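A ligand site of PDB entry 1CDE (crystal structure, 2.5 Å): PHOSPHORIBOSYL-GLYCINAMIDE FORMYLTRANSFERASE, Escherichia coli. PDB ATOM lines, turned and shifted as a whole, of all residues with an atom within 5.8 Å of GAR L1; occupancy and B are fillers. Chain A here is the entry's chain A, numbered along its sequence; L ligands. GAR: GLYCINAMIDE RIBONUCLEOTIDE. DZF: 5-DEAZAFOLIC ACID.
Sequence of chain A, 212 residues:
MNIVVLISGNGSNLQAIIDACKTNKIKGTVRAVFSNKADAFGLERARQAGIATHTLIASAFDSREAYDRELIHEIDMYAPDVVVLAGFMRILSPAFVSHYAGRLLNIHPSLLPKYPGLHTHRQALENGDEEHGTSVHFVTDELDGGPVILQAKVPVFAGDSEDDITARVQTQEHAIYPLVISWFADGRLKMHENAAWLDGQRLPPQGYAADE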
ATOM      1  N   GLY A   9      14.999 -10.804 -33.316  1.00  0.00           N
ATOM      2  CA  GLY A   9      15.141 -11.933 -32.414  1.00  0.00           C
ATOM      3  C   GLY A   9      13.919 -12.528 -31.724  1.00  0.00           C
ATOM      4  O   GLY A   9      13.011 -13.020 -32.403  1.00  0.00           O
ATOM      5  N   ASN A  10      13.805 -12.509 -30.389  1.00  0.00           N
ATOM      6  CA  ASN A  10      12.798 -13.362 -29.732  1.00  0.00           C
ATOM      7  C   ASN A  10      11.345 -12.992 -29.933  1.00  0.00           C
ATOM      8  O   ASN A  10      10.492 -13.845 -30.021  1.00  0.00           O
ATOM      9  CB  ASN A  10      13.098 -13.404 -28.253  1.00  0.00           C
ATOM     10  CG  ASN A  10      12.213 -14.413 -27.524  1.00  0.00           C
ATOM     11  OD1 ASN A  10      11.312 -14.041 -26.783  1.00  0.00           O
ATOM     12  ND2 ASN A  10      12.348 -15.707 -27.675  1.00  0.00           N
ATOM     13  N   GLY A  11      11.081 -11.701 -30.021  1.00  0.00           N
ATOM     14  CA  GLY A  11       9.755 -11.190 -30.271  1.00  0.00           C
ATOM     15  C   GLY A  11       8.808 -11.073 -29.091  1.00  0.00           C
ATOM     16  O   GLY A  11       7.595 -11.041 -29.283  1.00  0.00           O
ATOM     17  N   SER A  12       9.298 -10.888 -27.868  1.00  0.00           N
ATOM     18  CA  SER A  12       8.400 -10.706 -26.744  1.00  0.00           C
ATOM     19  C   SER A  12       7.729  -9.336 -26.746  1.00  0.00           C
ATOM     20  O   SER A  12       6.556  -9.203 -26.393  1.00  0.00           O
ATOM     21  CB  SER A  12       9.148 -10.937 -25.430  1.00  0.00           C
ATOM     22  OG  SER A  12       9.884  -9.791 -25.092  1.00  0.00           O
ATOM     23  N   ASN A  13       8.393  -8.246 -27.145  1.00  0.00           N
ATOM     24  CA  ASN A  13       7.722  -6.943 -27.302  1.00  0.00           C
ATOM     25  C   ASN A  13       6.675  -6.911 -28.448  1.00  0.00           C
ATOM     26  O   ASN A  13       5.596  -6.322 -28.312  1.00  0.00           O
ATOM     27  CB  ASN A  13       8.775  -5.905 -27.562  1.00  0.00           C
ATOM     28  CG  ASN A  13       9.371  -5.360 -26.287  1.00  0.00           C
ATOM     29  OD1 ASN A  13      10.306  -5.872 -25.711  1.00  0.00           O
ATOM     30  ND2 ASN A  13       8.894  -4.310 -25.715  1.00  0.00           N
ATOM     31  N   LEU A  14       6.992  -7.568 -29.569  1.00  0.00           N
ATOM     32  CA  LEU A  14       6.091  -7.835 -30.703  1.00  0.00           C
ATOM     33  C   LEU A  14       4.827  -8.531 -30.166  1.00  0.00           C
ATOM     34  O   LEU A  14       3.688  -8.103 -30.393  1.00  0.00           O
ATOM     35  CB  LEU A  14       6.769  -8.773 -31.715  1.00  0.00           C
ATOM     36  CG  LEU A  14       6.363  -9.110 -33.164  1.00  0.00           C
ATOM     37  CD1 LEU A  14       6.315 -10.619 -33.299  1.00  0.00           C
ATOM     38  CD2 LEU A  14       5.065  -8.458 -33.543  1.00  0.00           C
ATOM     39  N   ALA A  86      11.350  -3.109 -32.657  1.00  0.00           N
ATOM     40  CA  ALA A  86      11.225  -3.829 -31.424  1.00  0.00           C
ATOM     41  C   ALA A  86      12.223  -4.966 -31.403  1.00  0.00           C
ATOM     42  O   ALA A  86      11.949  -6.147 -31.599  1.00  0.00           O
ATOM     43  CB  ALA A  86       9.795  -4.375 -31.292  1.00  0.00           C
ATOM     44  N   GLY A  87      13.451  -4.561 -31.029  1.00  0.00           N
ATOM     45  CA  GLY A  87      14.617  -5.468 -31.035  1.00  0.00           C
ATOM     46  C   GLY A  87      15.378  -5.502 -32.364  1.00  0.00           C
ATOM     47  O   GLY A  87      16.033  -6.503 -32.641  1.00  0.00           O
ATOM     48  N   PHE A  88      15.361  -4.449 -33.185  1.00  0.00           N
ATOM     49  CA  PHE A  88      15.942  -4.536 -34.502  1.00  0.00           C
ATOM     50  C   PHE A  88      17.406  -4.148 -34.428  1.00  0.00           C
ATOM     51  O   PHE A  88      17.712  -2.989 -34.165  1.00  0.00           O
ATOM     52  CB  PHE A  88      15.155  -3.617 -35.431  1.00  0.00           C
ATOM     53  CG  PHE A  88      15.477  -3.762 -36.919  1.00  0.00           C
ATOM     54  CD1 PHE A  88      15.264  -4.962 -37.570  1.00  0.00           C
ATOM     55  CD2 PHE A  88      16.015  -2.671 -37.598  1.00  0.00           C
ATOM     56  CE1 PHE A  88      15.605  -5.064 -38.894  1.00  0.00           C
ATOM     57  CE2 PHE A  88      16.355  -2.784 -38.934  1.00  0.00           C
ATOM     58  CZ  PHE A  88      16.154  -3.981 -39.561  1.00  0.00           C
ATOM     59  N   MET A  89      18.333  -5.078 -34.612  1.00  0.00           N
ATOM     60  CA  MET A  89      19.734  -4.762 -34.498  1.00  0.00           C
ATOM     61  C   MET A  89      20.493  -4.157 -35.709  1.00  0.00           C
ATOM     62  O   MET A  89      21.471  -4.702 -36.214  1.00  0.00           O
ATOM     63  CB  MET A  89      20.370  -6.054 -34.030  1.00  0.00           C
ATOM     64  CG  MET A  89      20.016  -6.494 -32.582  1.00  0.00           C
ATOM     65  SD  MET A  89      20.013  -5.177 -31.325  1.00  0.00           S
ATOM     66  CE  MET A  89      19.115  -6.182 -30.183  1.00  0.00           C
ATOM     67  N   ASN A 106      11.167   3.509 -31.434  1.00  0.00           N
ATOM     68  CA  ASN A 106      12.048   2.461 -30.935  1.00  0.00           C
ATOM     69  C   ASN A 106      12.027   2.354 -29.401  1.00  0.00           C
ATOM     70  O   ASN A 106      11.809   3.338 -28.676  1.00  0.00           O
ATOM     71  CB  ASN A 106      13.467   2.724 -31.425  1.00  0.00           C
ATOM     72  CG  ASN A 106      14.540   1.697 -31.016  1.00  0.00           C
ATOM     73  OD1 ASN A 106      14.565   0.492 -31.304  1.00  0.00           O
ATOM     74  ND2 ASN A 106      15.508   2.168 -30.252  1.00  0.00           N
ATOM     75  N   ILE A 107      12.278   1.148 -28.913  1.00  0.00           N
ATOM     76  CA  ILE A 107      12.464   0.948 -27.513  1.00  0.00           C
ATOM     77  C   ILE A 107      13.922   0.573 -27.227  1.00  0.00           C
ATOM     78  O   ILE A 107      14.510  -0.387 -27.748  1.00  0.00           O
ATOM     79  CB  ILE A 107      11.460  -0.115 -27.044  1.00  0.00           C
ATOM     80  CG1 ILE A 107      11.545  -0.105 -25.538  1.00  0.00           C
ATOM     81  CG2 ILE A 107      11.734  -1.503 -27.486  1.00  0.00           C
ATOM     82  CD1 ILE A 107      10.220  -0.373 -24.799  1.00  0.00           C
ATOM     83  N   HIS A 108      14.569   1.402 -26.415  1.00  0.00           N
ATOM     84  CA  HIS A 108      15.975   1.217 -26.002  1.00  0.00           C
ATOM     85  C   HIS A 108      16.148   0.863 -24.494  1.00  0.00           C
ATOM     86  O   HIS A 108      15.644   1.614 -23.648  1.00  0.00           O
ATOM     87  CB  HIS A 108      16.774   2.534 -26.342  1.00  0.00           C
ATOM     88  CG  HIS A 108      18.280   2.403 -26.070  1.00  0.00           C
ATOM     89  ND1 HIS A 108      19.040   3.171 -25.283  1.00  0.00           N
ATOM     90  CD2 HIS A 108      19.076   1.366 -26.507  1.00  0.00           C
ATOM     91  CE1 HIS A 108      20.218   2.651 -25.215  1.00  0.00           C
ATOM     92  NE2 HIS A 108      20.217   1.573 -25.959  1.00  0.00           N
ATOM     93  N   PRO A 109      16.842  -0.189 -24.059  1.00  0.00           N
ATOM     94  CA  PRO A 109      16.869  -0.612 -22.661  1.00  0.00           C
ATOM     95  C   PRO A 109      17.808   0.124 -21.714  1.00  0.00           C
ATOM     96  O   PRO A 109      18.773  -0.416 -21.146  1.00  0.00           O
ATOM     97  CB  PRO A 109      17.131  -2.091 -22.777  1.00  0.00           C
ATOM     98  CG  PRO A 109      17.988  -2.240 -24.021  1.00  0.00           C
ATOM     99  CD  PRO A 109      17.549  -1.113 -24.921  1.00  0.00           C
ATOM    100  N   GLY A 117      23.971   2.789 -26.265  1.00  0.00           N
ATOM    101  CA  GLY A 117      24.460   1.861 -27.263  1.00  0.00           C
ATOM    102  C   GLY A 117      24.065   0.468 -26.946  1.00  0.00           C
ATOM    103  O   GLY A 117      22.931   0.221 -26.565  1.00  0.00           O
ATOM    104  N   HIS A 121      22.595  -3.151 -20.023  1.00  0.00           N
ATOM    105  CA  HIS A 121      22.388  -3.829 -18.729  1.00  0.00           C
ATOM    106  C   HIS A 121      23.700  -4.081 -17.997  1.00  0.00           C
ATOM    107  O   HIS A 121      23.861  -3.671 -16.833  1.00  0.00           O
ATOM    108  CB  HIS A 121      21.638  -5.141 -18.939  1.00  0.00           C
ATOM    109  CG  HIS A 121      20.260  -4.943 -19.585  1.00  0.00           C
ATOM    110  ND1 HIS A 121      19.310  -4.008 -19.470  1.00  0.00           N
ATOM    111  CD2 HIS A 121      19.754  -5.872 -20.478  1.00  0.00           C
ATOM    112  CE1 HIS A 121      18.287  -4.317 -20.212  1.00  0.00           C
ATOM    113  NE2 HIS A 121      18.570  -5.436 -20.811  1.00  0.00           N
ATOM    114  N   THR A 134      14.062   1.569 -18.968  1.00  0.00           N
ATOM    115  CA  THR A 134      13.851   1.437 -20.389  1.00  0.00           C
ATOM    116  C   THR A 134      13.253   2.671 -20.999  1.00  0.00           C
ATOM    117  O   THR A 134      12.588   3.425 -20.294  1.00  0.00           O
ATOM    118  CB  THR A 134      12.969   0.253 -20.670  1.00  0.00           C
ATOM    119  OG1 THR A 134      13.187  -0.024 -22.058  1.00  0.00           O
ATOM    120  CG2 THR A 134      11.535   0.482 -20.292  1.00  0.00           C
ATOM    121  N   ASP A 144      20.356   6.105 -31.037  1.00  0.00           N
ATOM    122  CA  ASP A 144      19.630   6.163 -29.767  1.00  0.00           C
ATOM    123  C   ASP A 144      19.390   7.518 -29.131  1.00  0.00           C
ATOM    124  O   ASP A 144      19.056   7.580 -27.954  1.00  0.00           O
ATOM    125  CB  ASP A 144      20.285   5.291 -28.747  1.00  0.00           C
ATOM    126  CG  ASP A 144      20.115   3.868 -29.194  1.00  0.00           C
ATOM    127  OD1 ASP A 144      19.035   3.457 -29.635  1.00  0.00           O
ATOM    128  OD2 ASP A 144      21.105   3.142 -29.110  1.00  0.00           O
ATOM    129  N   GLN A 170      12.465  -6.014 -19.244  1.00  0.00           N
ATOM    130  CA  GLN A 170      11.557  -6.464 -20.274  1.00  0.00           C
ATOM    131  C   GLN A 170      10.094  -6.414 -19.861  1.00  0.00           C
ATOM    132  O   GLN A 170       9.237  -5.991 -20.639  1.00  0.00           O
ATOM    133  CB  GLN A 170      11.864  -7.859 -20.699  1.00  0.00           C
ATOM    134  CG  GLN A 170      12.784  -7.583 -21.835  1.00  0.00           C
ATOM    135  CD  GLN A 170      13.107  -8.781 -22.731  1.00  0.00           C
ATOM    136  OE1 GLN A 170      12.860  -9.954 -22.438  1.00  0.00           O
ATOM    137  NE2 GLN A 170      13.660  -8.530 -23.901  1.00  0.00           N
ATOM    138  N   GLU A 173       8.883  -3.028 -20.454  1.00  0.00           N
ATOM    139  CA  GLU A 173       8.756  -2.769 -21.898  1.00  0.00           C
ATOM    140  C   GLU A 173       7.399  -3.256 -22.412  1.00  0.00           C
ATOM    141  O   GLU A 173       6.635  -2.544 -23.043  1.00  0.00           O
ATOM    142  CB  GLU A 173       9.826  -3.505 -22.657  1.00  0.00           C
ATOM    143  CG  GLU A 173      11.246  -3.123 -22.256  1.00  0.00           C
ATOM    144  CD  GLU A 173      12.351  -3.599 -23.167  1.00  0.00           C
ATOM    145  OE1 GLU A 173      12.298  -4.737 -23.674  1.00  0.00           O
ATOM    146  OE2 GLU A 173      13.264  -2.792 -23.350  1.00  0.00           O
ATOM    147  N   HIS A 174       7.028  -4.438 -22.007  1.00  0.00           N
ATOM    148  CA  HIS A 174       5.784  -5.013 -22.362  1.00  0.00           C
ATOM    149  C   HIS A 174       4.577  -4.237 -21.877  1.00  0.00           C
ATOM    150  O   HIS A 174       3.450  -4.495 -22.273  1.00  0.00           O
ATOM    151  CB  HIS A 174       5.660  -6.393 -21.817  1.00  0.00           C
ATOM    152  CG  HIS A 174       6.707  -7.309 -22.348  1.00  0.00           C
ATOM    153  ND1 HIS A 174       7.647  -7.052 -23.271  1.00  0.00           N
ATOM    154  CD2 HIS A 174       6.906  -8.597 -21.894  1.00  0.00           C
ATOM    155  CE1 HIS A 174       8.406  -8.114 -23.374  1.00  0.00           C
ATOM    156  NE2 HIS A 174       7.949  -9.036 -22.547  1.00  0.00           N
HETATM  157  C1  GAR L   1      14.249  -5.484 -26.063  1.00  0.00           C
HETATM  158  O6  GAR L   1      14.350  -5.878 -24.680  1.00  0.00           O
HETATM  159  C2  GAR L   1      14.750  -4.066 -26.409  1.00  0.00           C
HETATM  160  O8  GAR L   1      14.844  -3.196 -25.304  1.00  0.00           O
HETATM  161  C3  GAR L   1      16.152  -4.261 -26.990  1.00  0.00           C
HETATM  162  O4  GAR L   1      16.010  -5.515 -27.634  1.00  0.00           O
HETATM  163  C5  GAR L   1      15.164  -6.358 -26.855  1.00  0.00           C
HETATM  164  C10 GAR L   1      14.322  -7.262 -27.772  1.00  0.00           C
HETATM  165  O12 GAR L   1      13.440  -8.079 -26.997  1.00  0.00           O
HETATM  166  N19 GAR L   1      16.581  -3.235 -28.001  1.00  0.00           N
HETATM  167  C21 GAR L   1      17.861  -2.945 -28.353  1.00  0.00           C
HETATM  168  O22 GAR L   1      18.816  -3.436 -27.766  1.00  0.00           O
HETATM  169  C23 GAR L   1      18.106  -1.874 -29.469  1.00  0.00           C
HETATM  170  N24 GAR L   1      18.545  -0.492 -29.106  1.00  0.00           N
HETATM  171  P15 GAR L   1      12.489  -9.083 -27.691  1.00  0.00           P
HETATM  172  O16 GAR L   1      11.329  -8.101 -28.123  1.00  0.00           O
HETATM  173  O17 GAR L   1      11.964 -10.174 -26.657  1.00  0.00           O
HETATM  174  O18 GAR L   1      13.094  -9.724 -28.780  1.00  0.00           O
HETATM  175  N1  DZF L   2      18.922   3.794 -36.347  1.00  0.00           N
HETATM  176  C2  DZF L   2      18.957   5.150 -36.252  1.00  0.00           C
HETATM  177  NA2 DZF L   2      19.392   5.846 -37.244  1.00  0.00           N
HETATM  178  N3  DZF L   2      18.705   5.774 -35.132  1.00  0.00           N
HETATM  179  C4  DZF L   2      18.409   5.089 -34.055  1.00  0.00           C
HETATM  180  O4  DZF L   2      18.244   5.757 -33.028  1.00  0.00           O
HETATM  181  C4A DZF L   2      18.339   3.665 -34.124  1.00  0.00           C
HETATM  182  C5  DZF L   2      17.802   2.926 -33.000  1.00  0.00           C
HETATM  183  C6  DZF L   2      18.183   1.469 -33.024  1.00  0.00           C
HETATM  184  C7  DZF L   2      18.106   0.826 -34.401  1.00  0.00           C
HETATM  185  N8  DZF L   2      18.632   1.735 -35.445  1.00  0.00           N
HETATM  186  C8A DZF L   2      18.618   3.039 -35.311  1.00  0.00           C
HETATM  187  C9  DZF L   2      19.558   1.418 -32.376  1.00  0.00           C
HETATM  188  N10 DZF L   2      19.730  -0.021 -32.199  1.00  0.00           N
HETATM  189  C11 DZF L   2      23.036  -2.068 -33.464  1.00  0.00           C
HETATM  190  C12 DZF L   2      23.050  -0.670 -33.460  1.00  0.00           C
HETATM  191  C13 DZF L   2      22.004   0.055 -32.952  1.00  0.00           C
HETATM  192  C14 DZF L   2      20.909  -0.617 -32.426  1.00  0.00           C
HETATM  193  C15 DZF L   2      20.896  -2.005 -32.417  1.00  0.00           C
HETATM  194  C16 DZF L   2      21.945  -2.727 -32.933  1.00  0.00           C
HETATM  195  C   DZF L   2      24.154  -2.846 -33.963  1.00  0.00           C
HETATM  196  O   DZF L   2      24.173  -4.065 -34.129  1.00  0.00           O
HETATM  197  N   DZF L   2      25.197  -2.127 -34.301  1.00  0.00           N
HETATM  198  CA  DZF L   2      26.501  -2.622 -34.789  1.00  0.00           C
HETATM  199  CB  DZF L   2      26.360  -3.236 -36.251  1.00  0.00           C
HETATM  200  CG  DZF L   2      26.090  -2.362 -37.525  1.00  0.00           C
HETATM  201  CD  DZF L   2      24.614  -2.080 -37.764  1.00  0.00           C
HETATM  202  OE1 DZF L   2      24.122  -2.058 -38.886  1.00  0.00           O
HETATM  203  OE2 DZF L   2      23.882  -1.736 -36.694  1.00  0.00           O
HETATM  204  CT  DZF L   2      27.460  -1.398 -34.754  1.00  0.00           C
HETATM  205  O1  DZF L   2      28.522  -1.295 -35.371  1.00  0.00           O
HETATM  206  O2  DZF L   2      27.061  -0.411 -33.877  1.00  0.00           O
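Merely in contact with GAR L1: His 108, Pro 109, Ile 107, Met 89 and Gly 87. Hydrophobic or aromatic side chains that line GAR L1: Met 89, His 108 and Pro 109. The nearest printed residue that does not touch GAR L1 is Asp 144 (4.01 Å).
An oxygen (O17) of GAR L1 lies within hydrogen-bond range of the backbone NH of Ser 12. O17 of GAR L1 sits at hydrogen-bond distance from OG of Ser 12 (2.6 Å). N of Asn 13 lies within hydrogen-bond range of O16 of GAR L1, at 3.1 Å. An oxygen (O18) of GAR L1 is in hydrogen-bond range of the backbone NH of Gly 11 (3.1 Å). NE2 of Gln 170 is in hydrogen-bond range of O6 of GAR L1 (2.8 Å). The side-chain amide oxygen (OD1) of Asn 13 lies close to an oxygen (O16) of GAR L1, at 3.4 Å. The backbone NH (N) of Asn 10 lies within hydrogen-bond range of an oxygen (O18) of GAR L1 (3.3 Å). The backbone NH of Asp 144 lies within hydrogen-bond range of an oxygen (O4) of DZF L2. The side-chain carboxylate (OE2) of Glu 173 sits at hydrogen-bond distance from an oxygen (O8) of GAR L1 (2.5 Å).
A nitrogen (N24) of GAR L1 sits close to a nitrogen (N10) of DZF L2 (3.3 Å).
OD1 of Asn 13 sits close to OE1 of Glu 173 (3.1 Å). A ring nitrogen (NE2) of His 108 is in hydrogen-bond range of the backbone carbonyl oxygen (O) of Gly 117, 3.1 Å away. OG of Ser 12 lies close to NE2 of His 174 (3.3 Å). The side-chain carboxylate (OE2) of Glu 173 lies within hydrogen-bond range of the side-chain hydroxyl (OG1) of Thr 134 (3.1 Å). O of His 108 sits at hydrogen-bond distance from OG1 of Thr 134. The backbone carbonyl oxygen of Gln 170 is in hydrogen-bond range of a ring nitrogen (ND1) of His 174, 3.3 Å away.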
